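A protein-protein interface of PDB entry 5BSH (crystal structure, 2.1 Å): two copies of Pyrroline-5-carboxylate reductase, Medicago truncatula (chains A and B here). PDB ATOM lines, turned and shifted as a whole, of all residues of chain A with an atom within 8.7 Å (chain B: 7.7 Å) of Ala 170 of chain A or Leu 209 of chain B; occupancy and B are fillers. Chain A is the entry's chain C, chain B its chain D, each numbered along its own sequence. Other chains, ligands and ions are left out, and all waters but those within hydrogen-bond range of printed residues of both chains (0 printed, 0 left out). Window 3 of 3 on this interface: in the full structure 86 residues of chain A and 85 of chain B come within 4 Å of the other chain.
Among the printed residues, merely in contact across the chains: Tyr 174 of chain A with Gly 204 of chain B, Trp 168 of chain A with Ser 212 of chain B, Ala 177 of chain A with Leu 205 of chain B, Leu 181 of chain A with Ala 210 of chain B, Tyr 174 of chain A with Leu 205 of chain B, Ile 178 of chain A with Leu 205 of chain B, Trp 168 of chain A with Leu 209 of chain B, Tyr 174 of chain A with Pro 206 of chain B, Trp 168 of chain A with Leu 213 of chain B, Ala 170 of chain A with Leu 209 of chain B, Val 142 of chain A with Leu 213 of chain B, Leu 181 of chain A with Leu 205 of chain B and Leu 181 of chain A with Leu 213 of chain B.
No position is printed for both chains.
Of chain B, only Leu 209 comes within 4 Å of Ala 170 of chain A.
Printed residues of chain B within 4 Å of Ile 178 of chain A: Leu 205.
Of the printed residues of chain B, Leu 181 of chain A touches Leu 205 (3.9 Å), Ala 210 (3.6 Å) and Leu 213 (3.96 Å).
Leu 209 of chain B touches just these residues of chain A: Trp 168 (3.8 Å) and Ala 170 (3.8 Å).
Ala 210 of chain B touches just one residue of chain A: Leu 181 (3.6 Å).
The nearest printed residue of chain B that does not touch Ala 177 of chain A is Gly 200 of chain B (4.9 Å).
The backbone carbonyl oxygen (O) of Ser 141 of chain A lies within hydrogen-bond range of the backbone NH (N) of Trp 168 of chain A.
OG of Ser 212 of chain B lies within hydrogen-bond range of O of Asp 208 of chain B, at 2.9 Å.
The backbone carbonyl oxygen (O) of Gly 200 of chain B is in hydrogen-bond range of the backbone NH (N) of Leu 205 of chain B (3.0 Å).
The backbone carbonyl oxygen of Met 143 of chain A is in hydrogen-bond range of the backbone NH of Ala 170 of chain A (2.9 Å).
N of Met 143 of chain A is in hydrogen-bond range of O of Trp 168 of chain A.
The backbone carbonyl oxygen (O) of Ile 178 of chain A lies close to the side-chain hydroxyl (OG) of Ser 182 of chain A (3.2 Å).
Hydrophobic or aromatic side chains of chain B that line the printed part of chain A: Leu 205, Pro 206, Leu 209 and Leu 213.
Hydrophobic or aromatic side chains of chain A that line the printed part of chain B: Val 142, Trp 168, Ala 170, Tyr 174, Ala 177, Ile 178 and Leu 181.
Among the printed residues, no Asp or Glu carboxylate lies within 4 Å of a Lys or Arg side-chain nitrogen of the other chain.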
ATOM      1  N   MET A 113       1.389  -9.755 -11.074  1.00  0.00           N
ATOM      2  CA  MET A 113       1.325  -8.674 -10.074  1.00  0.00           C
ATOM      3  C   MET A 113       0.324  -8.996  -8.958  1.00  0.00           C
ATOM      4  O   MET A 113       0.607  -8.804  -7.779  1.00  0.00           O
ATOM      5  CB  MET A 113       0.922  -7.335 -10.748  1.00  0.00           C
ATOM      6  CG  MET A 113       0.925  -6.139  -9.794  1.00  0.00           C
ATOM      7  SD  MET A 113       2.494  -5.981  -8.867  1.00  0.00           S
ATOM      8  CE  MET A 113       3.534  -5.293 -10.156  1.00  0.00           C
ATOM      9  N   ILE A 126       6.697  -3.427  -8.008  1.00  0.00           N
ATOM     10  CA  ILE A 126       6.892  -3.297  -9.415  1.00  0.00           C
ATOM     11  C   ILE A 126       7.412  -4.619  -9.959  1.00  0.00           C
ATOM     12  O   ILE A 126       8.250  -5.309  -9.356  1.00  0.00           O
ATOM     13  CB  ILE A 126       7.817  -2.125  -9.760  1.00  0.00           C
ATOM     14  CG1 ILE A 126       7.092  -0.798  -9.458  1.00  0.00           C
ATOM     15  CG2 ILE A 126       8.207  -2.155 -11.247  1.00  0.00           C
ATOM     16  CD1 ILE A 126       7.975   0.429  -9.603  1.00  0.00           C
ATOM     17  N   ARG A 127       6.901  -4.969 -11.115  1.00  0.00           N
ATOM     18  CA  ARG A 127       7.314  -6.222 -11.800  1.00  0.00           C
ATOM     19  C   ARG A 127       8.063  -5.822 -13.051  1.00  0.00           C
ATOM     20  O   ARG A 127       7.640  -4.902 -13.791  1.00  0.00           O
ATOM     21  CB  ARG A 127       6.134  -7.105 -12.195  1.00  0.00           C
ATOM     22  CG  ARG A 127       6.561  -8.381 -12.935  1.00  0.00           C
ATOM     23  CD  ARG A 127       5.340  -9.111 -13.437  1.00  0.00           C
ATOM     24  NE  ARG A 127       5.659 -10.276 -14.230  1.00  0.00           N
ATOM     25  CZ  ARG A 127       4.760 -10.979 -14.888  1.00  0.00           C
ATOM     26  NH1 ARG A 127       3.484 -10.654 -14.830  1.00  0.00           N
ATOM     27  NH2 ARG A 127       5.124 -12.032 -15.580  1.00  0.00           N
ATOM     28  N   VAL A 128       9.205  -6.466 -13.224  1.00  0.00           N
ATOM     29  CA  VAL A 128      10.056  -6.232 -14.385  1.00  0.00           C
ATOM     30  C   VAL A 128      10.373  -7.548 -15.021  1.00  0.00           C
ATOM     31  O   VAL A 128      10.663  -8.565 -14.353  1.00  0.00           O
ATOM     32  CB  VAL A 128      11.374  -5.511 -14.011  1.00  0.00           C
ATOM     33  CG1 VAL A 128      12.186  -5.231 -15.269  1.00  0.00           C
ATOM     34  CG2 VAL A 128      11.057  -4.180 -13.383  1.00  0.00           C
ATOM     35  N   ALA A 140      16.124  -5.827 -23.296  1.00  0.00           N
ATOM     36  CA  ALA A 140      14.794  -5.272 -23.564  1.00  0.00           C
ATOM     37  C   ALA A 140      13.936  -5.654 -22.371  1.00  0.00           C
ATOM     38  O   ALA A 140      13.633  -6.832 -22.161  1.00  0.00           O
ATOM     39  CB  ALA A 140      14.204  -5.785 -24.868  1.00  0.00           C
ATOM     40  N   SER A 141      13.569  -4.651 -21.586  1.00  0.00           N
ATOM     41  CA  SER A 141      12.816  -4.894 -20.373  1.00  0.00           C
ATOM     42  C   SER A 141      11.458  -4.202 -20.413  1.00  0.00           C
ATOM     43  O   SER A 141      11.300  -3.155 -21.031  1.00  0.00           O
ATOM     44  CB  SER A 141      13.600  -4.369 -19.187  1.00  0.00           C
ATOM     45  OG  SER A 141      14.799  -5.076 -19.044  1.00  0.00           O
ATOM     46  N   VAL A 142      10.492  -4.785 -19.737  1.00  0.00           N
ATOM     47  CA  VAL A 142       9.218  -4.121 -19.519  1.00  0.00           C
ATOM     48  C   VAL A 142       8.827  -4.174 -18.046  1.00  0.00           C
ATOM     49  O   VAL A 142       9.114  -5.148 -17.334  1.00  0.00           O
ATOM     50  CB  VAL A 142       8.090  -4.686 -20.304  1.00  0.00           C
ATOM     51  CG1 VAL A 142       8.422  -4.732 -21.766  1.00  0.00           C
ATOM     52  CG2 VAL A 142       7.901  -6.111 -19.878  1.00  0.00           C
ATOM     53  N   MET A 143       8.174  -3.112 -17.606  1.00  0.00           N
ATOM     54  CA  MET A 143       7.721  -3.013 -16.219  1.00  0.00           C
ATOM     55  C   MET A 143       6.212  -2.783 -16.106  1.00  0.00           C
ATOM     56  O   MET A 143       5.617  -2.062 -16.920  1.00  0.00           O
ATOM     57  CB  MET A 143       8.489  -1.942 -15.437  1.00  0.00           C
ATOM     58  CG  MET A 143       8.066  -0.503 -15.651  1.00  0.00           C
ATOM     59  SD  MET A 143       8.676   0.600 -14.319  1.00  0.00           S
ATOM     60  CE  MET A 143      10.344   0.754 -14.784  1.00  0.00           C
ATOM     61  N   SER A 144       5.605  -3.439 -15.108  1.00  0.00           N
ATOM     62  CA  SER A 144       4.205  -3.165 -14.711  1.00  0.00           C
ATOM     63  C   SER A 144       4.172  -2.737 -13.233  1.00  0.00           C
ATOM     64  O   SER A 144       5.068  -3.121 -12.461  1.00  0.00           O
ATOM     65  CB  SER A 144       3.297  -4.375 -14.951  1.00  0.00           C
ATOM     66  OG  SER A 144       3.760  -5.452 -14.159  1.00  0.00           O
ATOM     67  N   LEU A 145       3.201  -1.875 -12.892  1.00  0.00           N
ATOM     68  CA  LEU A 145       3.150  -1.198 -11.577  1.00  0.00           C
ATOM     69  C   LEU A 145       2.064  -1.784 -10.740  1.00  0.00           C
ATOM     70  O   LEU A 145       0.936  -1.909 -11.200  1.00  0.00           O
ATOM     71  CB  LEU A 145       2.846   0.284 -11.740  1.00  0.00           C
ATOM     72  CG  LEU A 145       3.756   1.128 -12.630  1.00  0.00           C
ATOM     73  CD1 LEU A 145       3.492   2.618 -12.422  1.00  0.00           C
ATOM     74  CD2 LEU A 145       5.222   0.833 -12.354  1.00  0.00           C
ATOM     75  N   GLY A 146       2.400  -2.138  -9.509  1.00  0.00           N
ATOM     76  CA  GLY A 146       1.375  -2.475  -8.525  1.00  0.00           C
ATOM     77  C   GLY A 146       0.501  -1.271  -8.217  1.00  0.00           C
ATOM     78  O   GLY A 146       0.845  -0.138  -8.562  1.00  0.00           O
ATOM     79  N   ILE A 167      14.025   0.110 -21.202  1.00  0.00           N
ATOM     80  CA  ILE A 167      12.866  -0.291 -20.434  1.00  0.00           C
ATOM     81  C   ILE A 167      11.613   0.490 -20.777  1.00  0.00           C
ATOM     82  O   ILE A 167      11.632   1.680 -21.034  1.00  0.00           O
ATOM     83  CB  ILE A 167      13.163  -0.250 -18.910  1.00  0.00           C
ATOM     84  CG1 ILE A 167      11.939  -0.757 -18.146  1.00  0.00           C
ATOM     85  CG2 ILE A 167      13.628   1.102 -18.484  1.00  0.00           C
ATOM     86  CD1 ILE A 167      12.310  -1.632 -16.963  1.00  0.00           C
ATOM     87  N   TRP A 168      10.527  -0.256 -20.921  1.00  0.00           N
ATOM     88  CA  TRP A 168       9.230   0.281 -21.282  1.00  0.00           C
ATOM     89  C   TRP A 168       8.202  -0.125 -20.259  1.00  0.00           C
ATOM     90  O   TRP A 168       8.407  -1.087 -19.522  1.00  0.00           O
ATOM     91  CB  TRP A 168       8.802  -0.233 -22.657  1.00  0.00           C
ATOM     92  CG  TRP A 168       9.640   0.328 -23.717  1.00  0.00           C
ATOM     93  CD1 TRP A 168       9.434   1.498 -24.378  1.00  0.00           C
ATOM     94  CD2 TRP A 168      10.815  -0.258 -24.309  1.00  0.00           C
ATOM     95  NE1 TRP A 168      10.390   1.676 -25.341  1.00  0.00           N
ATOM     96  CE2 TRP A 168      11.260   0.629 -25.318  1.00  0.00           C
ATOM     97  CE3 TRP A 168      11.490  -1.467 -24.137  1.00  0.00           C
ATOM     98  CZ2 TRP A 168      12.357   0.355 -26.129  1.00  0.00           C
ATOM     99  CZ3 TRP A 168      12.605  -1.711 -24.895  1.00  0.00           C
ATOM    100  CH2 TRP A 168      13.031  -0.808 -25.888  1.00  0.00           C
ATOM    101  N   LYS A 169       7.078   0.580 -20.247  1.00  0.00           N
ATOM    102  CA  LYS A 169       5.982   0.270 -19.346  1.00  0.00           C
ATOM    103  C   LYS A 169       4.925  -0.510 -20.079  1.00  0.00           C
ATOM    104  O   LYS A 169       4.660  -0.249 -21.225  1.00  0.00           O
ATOM    105  CB  LYS A 169       5.422   1.543 -18.746  1.00  0.00           C
ATOM    106  CG  LYS A 169       6.494   2.204 -17.886  1.00  0.00           C
ATOM    107  CD  LYS A 169       6.060   3.433 -17.121  1.00  0.00           C
ATOM    108  CE  LYS A 169       7.294   4.181 -16.636  1.00  0.00           C
ATOM    109  NZ  LYS A 169       6.901   5.242 -15.682  1.00  0.00           N
ATOM    110  N   ALA A 170       4.342  -1.499 -19.419  1.00  0.00           N
ATOM    111  CA  ALA A 170       3.181  -2.196 -19.964  1.00  0.00           C
ATOM    112  C   ALA A 170       2.288  -2.848 -18.908  1.00  0.00           C
ATOM    113  O   ALA A 170       2.779  -3.174 -17.857  1.00  0.00           O
ATOM    114  CB  ALA A 170       3.675  -3.253 -20.921  1.00  0.00           C
ATOM    115  N   ASP A 171       1.001  -3.035 -19.223  1.00  0.00           N
ATOM    116  CA  ASP A 171       0.069  -3.701 -18.332  1.00  0.00           C
ATOM    117  C   ASP A 171       0.550  -5.096 -18.124  1.00  0.00           C
ATOM    118  O   ASP A 171       0.995  -5.742 -19.076  1.00  0.00           O
ATOM    119  CB  ASP A 171      -1.333  -3.851 -18.946  1.00  0.00           C
ATOM    120  CG  ASP A 171      -2.219  -2.638 -18.763  1.00  0.00           C
ATOM    121  OD1 ASP A 171      -1.727  -1.489 -18.783  1.00  0.00           O
ATOM    122  OD2 ASP A 171      -3.445  -2.819 -18.573  1.00  0.00           O
ATOM    123  N   ASP A 172       0.368  -5.569 -16.903  1.00  0.00           N
ATOM    124  CA  ASP A 172       0.691  -6.924 -16.526  1.00  0.00           C
ATOM    125  C   ASP A 172       0.085  -7.934 -17.434  1.00  0.00           C
ATOM    126  O   ASP A 172       0.683  -8.971 -17.689  1.00  0.00           O
ATOM    127  CB  ASP A 172       0.210  -7.184 -15.087  1.00  0.00           C
ATOM    128  CG  ASP A 172       1.088  -8.178 -14.351  1.00  0.00           C
ATOM    129  OD1 ASP A 172       2.300  -7.914 -14.185  1.00  0.00           O
ATOM    130  OD2 ASP A 172       0.587  -9.232 -13.958  1.00  0.00           O
ATOM    131  N   LYS A 173      -1.100  -7.674 -17.958  1.00  0.00           N
ATOM    132  CA  LYS A 173      -1.712  -8.684 -18.824  1.00  0.00           C
ATOM    133  C   LYS A 173      -0.902  -8.980 -20.121  1.00  0.00           C
ATOM    134  O   LYS A 173      -1.162  -9.944 -20.783  1.00  0.00           O
ATOM    135  CB  LYS A 173      -3.142  -8.284 -19.193  1.00  0.00           C
ATOM    136  CG  LYS A 173      -3.155  -7.162 -20.193  1.00  0.00           C
ATOM    137  CD  LYS A 173      -4.560  -6.791 -20.576  1.00  0.00           C
ATOM    138  CE  LYS A 173      -4.554  -5.366 -21.104  1.00  0.00           C
ATOM    139  NZ  LYS A 173      -5.878  -5.031 -21.657  1.00  0.00           N
ATOM    140  N   TYR A 174       0.018  -8.106 -20.514  1.00  0.00           N
ATOM    141  CA  TYR A 174       0.762  -8.307 -21.755  1.00  0.00           C
ATOM    142  C   TYR A 174       1.968  -9.210 -21.553  1.00  0.00           C
ATOM    143  O   TYR A 174       2.643  -9.556 -22.526  1.00  0.00           O
ATOM    144  CB  TYR A 174       1.207  -6.977 -22.398  1.00  0.00           C
ATOM    145  CG  TYR A 174       0.086  -6.108 -22.856  1.00  0.00           C
ATOM    146  CD1 TYR A 174      -0.863  -6.581 -23.723  1.00  0.00           C
ATOM    147  CD2 TYR A 174      -0.028  -4.774 -22.421  1.00  0.00           C
ATOM    148  CE1 TYR A 174      -1.908  -5.785 -24.146  1.00  0.00           C
ATOM    149  CE2 TYR A 174      -1.084  -3.975 -22.827  1.00  0.00           C
ATOM    150  CZ  TYR A 174      -2.009  -4.481 -23.709  1.00  0.00           C
ATOM    151  OH  TYR A 174      -3.068  -3.747 -24.118  1.00  0.00           O
ATOM    152  N   PHE A 175       2.259  -9.588 -20.323  1.00  0.00           N
ATOM    153  CA  PHE A 175       3.570 -10.234 -20.004  1.00  0.00           C
ATOM    154  C   PHE A 175       3.822 -11.651 -20.640  1.00  0.00           C
ATOM    155  O   PHE A 175       4.935 -11.981 -21.069  1.00  0.00           O
ATOM    156  CB  PHE A 175       3.840 -10.199 -18.475  1.00  0.00           C
ATOM    157  CG  PHE A 175       4.489  -8.901 -18.011  1.00  0.00           C
ATOM    158  CD1 PHE A 175       3.904  -7.686 -18.285  1.00  0.00           C
ATOM    159  CD2 PHE A 175       5.713  -8.900 -17.400  1.00  0.00           C
ATOM    160  CE1 PHE A 175       4.504  -6.478 -17.919  1.00  0.00           C
ATOM    161  CE2 PHE A 175       6.303  -7.713 -17.011  1.00  0.00           C
ATOM    162  CZ  PHE A 175       5.701  -6.497 -17.253  1.00  0.00           C
ATOM    163  N   ALA A 177       2.723 -12.528 -23.797  1.00  0.00           N
ATOM    164  CA  ALA A 177       3.139 -12.161 -25.108  1.00  0.00           C
ATOM    165  C   ALA A 177       4.562 -11.512 -25.149  1.00  0.00           C
ATOM    166  O   ALA A 177       5.344 -11.696 -26.119  1.00  0.00           O
ATOM    167  CB  ALA A 177       2.131 -11.196 -25.686  1.00  0.00           C
ATOM    168  N   ILE A 178       4.857 -10.659 -24.157  1.00  0.00           N
ATOM    169  CA  ILE A 178       6.157 -10.040 -24.140  1.00  0.00           C
ATOM    170  C   ILE A 178       7.213 -11.148 -24.039  1.00  0.00           C
ATOM    171  O   ILE A 178       8.261 -11.096 -24.649  1.00  0.00           O
ATOM    172  CB  ILE A 178       6.258  -9.056 -22.961  1.00  0.00           C
ATOM    173  CG1 ILE A 178       5.356  -7.887 -23.261  1.00  0.00           C
ATOM    174  CG2 ILE A 178       7.705  -8.641 -22.765  1.00  0.00           C
ATOM    175  CD1 ILE A 178       5.019  -6.976 -22.071  1.00  0.00           C
ATOM    176  N   LEU A 181       8.248 -12.596 -27.253  1.00  0.00           N
ATOM    177  CA  LEU A 181       8.910 -11.640 -28.151  1.00  0.00           C
ATOM    178  C   LEU A 181      10.294 -11.275 -27.571  1.00  0.00           C
ATOM    179  O   LEU A 181      11.300 -11.716 -28.084  1.00  0.00           O
ATOM    180  CB  LEU A 181       8.031 -10.428 -28.384  1.00  0.00           C
ATOM    181  CG  LEU A 181       8.623  -9.270 -29.202  1.00  0.00           C
ATOM    182  CD1 LEU A 181       9.216  -9.786 -30.508  1.00  0.00           C
ATOM    183  CD2 LEU A 181       7.645  -8.205 -29.506  1.00  0.00           C
ATOM    184  N   SER A 182      10.329 -10.481 -26.493  1.00  0.00           N
ATOM    185  CA  SER A 182      11.639 -10.052 -25.954  1.00  0.00           C
ATOM    186  C   SER A 182      12.300 -11.086 -25.108  1.00  0.00           C
ATOM    187  O   SER A 182      13.529 -11.142 -25.066  1.00  0.00           O
ATOM    188  CB  SER A 182      11.506  -8.719 -25.161  1.00  0.00           C
ATOM    189  OG  SER A 182      10.494  -8.857 -24.190  1.00  0.00           O
ATOM    190  N   ALA B 197       7.565  -7.761 -34.736  1.00  0.00           N
ATOM    191  CA  ALA B 197       6.592  -6.830 -34.224  1.00  0.00           C
ATOM    192  C   ALA B 197       5.181  -7.312 -34.561  1.00  0.00           C
ATOM    193  O   ALA B 197       4.294  -7.261 -33.728  1.00  0.00           O
ATOM    194  CB  ALA B 197       6.886  -5.447 -34.771  1.00  0.00           C
ATOM    195  N   GLY B 200       4.218  -9.967 -32.313  1.00  0.00           N
ATOM    196  CA  GLY B 200       3.815  -9.477 -31.006  1.00  0.00           C
ATOM    197  C   GLY B 200       2.406  -8.954 -30.990  1.00  0.00           C
ATOM    198  O   GLY B 200       1.594  -9.342 -30.150  1.00  0.00           O
ATOM    199  N   VAL B 201       2.048  -8.205 -32.027  1.00  0.00           N
ATOM    200  CA  VAL B 201       0.729  -7.713 -32.147  1.00  0.00           C
ATOM    201  C   VAL B 201      -0.262  -8.884 -32.295  1.00  0.00           C
ATOM    202  O   VAL B 201      -1.416  -8.841 -31.793  1.00  0.00           O
ATOM    203  CB  VAL B 201       0.631  -6.704 -33.326  1.00  0.00           C
ATOM    204  CG1 VAL B 201      -0.795  -6.243 -33.585  1.00  0.00           C
ATOM    205  CG2 VAL B 201       1.478  -5.487 -33.061  1.00  0.00           C
ATOM    206  N   GLY B 204      -1.281 -10.069 -29.180  1.00  0.00           N
ATOM    207  CA  GLY B 204      -2.030  -9.178 -28.268  1.00  0.00           C
ATOM    208  C   GLY B 204      -1.276  -7.945 -27.778  1.00  0.00           C
ATOM    209  O   GLY B 204      -1.879  -7.103 -27.101  1.00  0.00           O
ATOM    210  N   LEU B 205      -0.018  -7.779 -28.171  1.00  0.00           N
ATOM    211  CA  LEU B 205       0.689  -6.580 -27.812  1.00  0.00           C
ATOM    212  C   LEU B 205       0.317  -5.323 -28.589  1.00  0.00           C
ATOM    213  O   LEU B 205       0.096  -5.355 -29.794  1.00  0.00           O
ATOM    214  CB  LEU B 205       2.205  -6.744 -27.970  1.00  0.00           C
ATOM    215  CG  LEU B 205       2.882  -7.852 -27.258  1.00  0.00           C
ATOM    216  CD1 LEU B 205       4.350  -7.770 -27.528  1.00  0.00           C
ATOM    217  CD2 LEU B 205       2.606  -7.633 -25.772  1.00  0.00           C
ATOM    218  N   PRO B 206       0.357  -4.179 -27.907  1.00  0.00           N
ATOM    219  CA  PRO B 206       0.325  -2.917 -28.639  1.00  0.00           C
ATOM    220  C   PRO B 206       1.476  -2.767 -29.628  1.00  0.00           C
ATOM    221  O   PRO B 206       2.610  -3.197 -29.333  1.00  0.00           O
ATOM    222  CB  PRO B 206       0.497  -1.819 -27.517  1.00  0.00           C
ATOM    223  CG  PRO B 206       0.142  -2.495 -26.251  1.00  0.00           C
ATOM    224  CD  PRO B 206       0.508  -3.980 -26.444  1.00  0.00           C
ATOM    225  N   ARG B 207       1.170  -2.087 -30.737  1.00  0.00           N
ATOM    226  CA  ARG B 207       2.101  -1.931 -31.819  1.00  0.00           C
ATOM    227  C   ARG B 207       3.383  -1.214 -31.447  1.00  0.00           C
ATOM    228  O   ARG B 207       4.478  -1.672 -31.791  1.00  0.00           O
ATOM    229  CB  ARG B 207       1.402  -1.158 -32.940  1.00  0.00           C
ATOM    230  CG  ARG B 207       2.307  -0.767 -34.091  1.00  0.00           C
ATOM    231  CD  ARG B 207       2.956  -1.956 -34.803  1.00  0.00           C
ATOM    232  NE  ARG B 207       1.939  -2.798 -35.457  1.00  0.00           N
ATOM    233  CZ  ARG B 207       2.244  -3.909 -36.184  1.00  0.00           C
ATOM    234  NH1 ARG B 207       3.515  -4.276 -36.386  1.00  0.00           N
ATOM    235  NH2 ARG B 207       1.268  -4.603 -36.797  1.00  0.00           N
ATOM    236  N   ASP B 208       3.280  -0.066 -30.774  1.00  0.00           N
ATOM    237  CA  ASP B 208       4.501   0.679 -30.467  1.00  0.00           C
ATOM    238  C   ASP B 208       5.400  -0.090 -29.565  1.00  0.00           C
ATOM    239  O   ASP B 208       6.625  -0.165 -29.768  1.00  0.00           O
ATOM    240  CB  ASP B 208       4.161   2.025 -29.818  1.00  0.00           C
ATOM    241  CG  ASP B 208       3.463   2.983 -30.780  1.00  0.00           C
ATOM    242  OD1 ASP B 208       3.527   2.808 -32.032  1.00  0.00           O
ATOM    243  OD2 ASP B 208       2.825   3.933 -30.264  1.00  0.00           O
ATOM    244  N   LEU B 209       4.814  -0.735 -28.565  1.00  0.00           N
ATOM    245  CA  LEU B 209       5.641  -1.618 -27.693  1.00  0.00           C
ATOM    246  C   LEU B 209       6.288  -2.781 -28.491  1.00  0.00           C
ATOM    247  O   LEU B 209       7.449  -3.157 -28.294  1.00  0.00           O
ATOM    248  CB  LEU B 209       4.789  -2.208 -26.563  1.00  0.00           C
ATOM    249  CG  LEU B 209       5.490  -3.111 -25.571  1.00  0.00           C
ATOM    250  CD1 LEU B 209       6.541  -2.297 -24.823  1.00  0.00           C
ATOM    251  CD2 LEU B 209       4.515  -3.729 -24.590  1.00  0.00           C
ATOM    252  N   ALA B 210       5.461  -3.420 -29.329  1.00  0.00           N
ATOM    253  CA  ALA B 210       5.942  -4.577 -30.084  1.00  0.00           C
ATOM    254  C   ALA B 210       7.160  -4.212 -30.949  1.00  0.00           C
ATOM    255  O   ALA B 210       8.104  -4.927 -30.981  1.00  0.00           O
ATOM    256  CB  ALA B 210       4.813  -5.114 -30.947  1.00  0.00           C
ATOM    257  N   LEU B 211       7.079  -3.083 -31.640  1.00  0.00           N
ATOM    258  CA  LEU B 211       8.127  -2.666 -32.444  1.00  0.00           C
ATOM    259  C   LEU B 211       9.372  -2.312 -31.631  1.00  0.00           C
ATOM    260  O   LEU B 211      10.488  -2.719 -31.983  1.00  0.00           O
ATOM    261  CB  LEU B 211       7.664  -1.515 -33.287  1.00  0.00           C
ATOM    262  CG  LEU B 211       8.689  -1.004 -34.274  1.00  0.00           C
ATOM    263  CD1 LEU B 211       9.177  -2.108 -35.220  1.00  0.00           C
ATOM    264  CD2 LEU B 211       8.016   0.113 -35.088  1.00  0.00           C
ATOM    265  N   SER B 212       9.192  -1.518 -30.586  1.00  0.00           N
ATOM    266  CA  SER B 212      10.309  -1.196 -29.686  1.00  0.00           C
ATOM    267  C   SER B 212      10.946  -2.408 -29.169  1.00  0.00           C
ATOM    268  O   SER B 212      12.178  -2.502 -29.122  1.00  0.00           O
ATOM    269  CB  SER B 212       9.824  -0.338 -28.494  1.00  0.00           C
ATOM    270  OG  SER B 212       9.250   0.882 -28.965  1.00  0.00           O
ATOM    271  N   LEU B 213      10.142  -3.386 -28.739  1.00  0.00           N
ATOM    272  CA  LEU B 213      10.773  -4.622 -28.192  1.00  0.00           C
ATOM    273  C   LEU B 213      11.522  -5.371 -29.254  1.00  0.00           C
ATOM    274  O   LEU B 213      12.574  -5.987 -29.008  1.00  0.00           O
ATOM    275  CB  LEU B 213       9.752  -5.517 -27.511  1.00  0.00           C
ATOM    276  CG  LEU B 213       9.133  -5.008 -26.226  1.00  0.00           C
ATOM    277  CD1 LEU B 213       8.037  -5.933 -25.750  1.00  0.00           C
ATOM    278  CD2 LEU B 213      10.202  -4.860 -25.136  1.00  0.00           C
ATOM    279  N   ALA B 214      10.933  -5.408 -30.455  1.00  0.00           N
ATOM    280  CA  ALA B 214      11.526  -6.241 -31.540  1.00  0.00           C
ATOM    281  C   ALA B 214      12.920  -5.702 -31.873  1.00  0.00           C
ATOM    282  O   ALA B 214      13.901  -6.417 -31.898  1.00  0.00           O
ATOM    283  CB  ALA B 214      10.628  -6.177 -32.751  1.00  0.00           C
ATOM    284  N   SER B 215      12.991  -4.389 -32.095  1.00  0.00           N
ATOM    285  CA  SER B 215      14.265  -3.772 -32.418  1.00  0.00           C
ATOM    286  C   SER B 215      15.318  -3.988 -31.336  1.00  0.00           C
ATOM    287  O   SER B 215      16.446  -4.365 -31.619  1.00  0.00           O
ATOM    288  CB  SER B 215      14.082  -2.253 -32.695  1.00  0.00           C
ATOM    289  OG  SER B 215      13.259  -2.085 -33.823  1.00  0.00           O
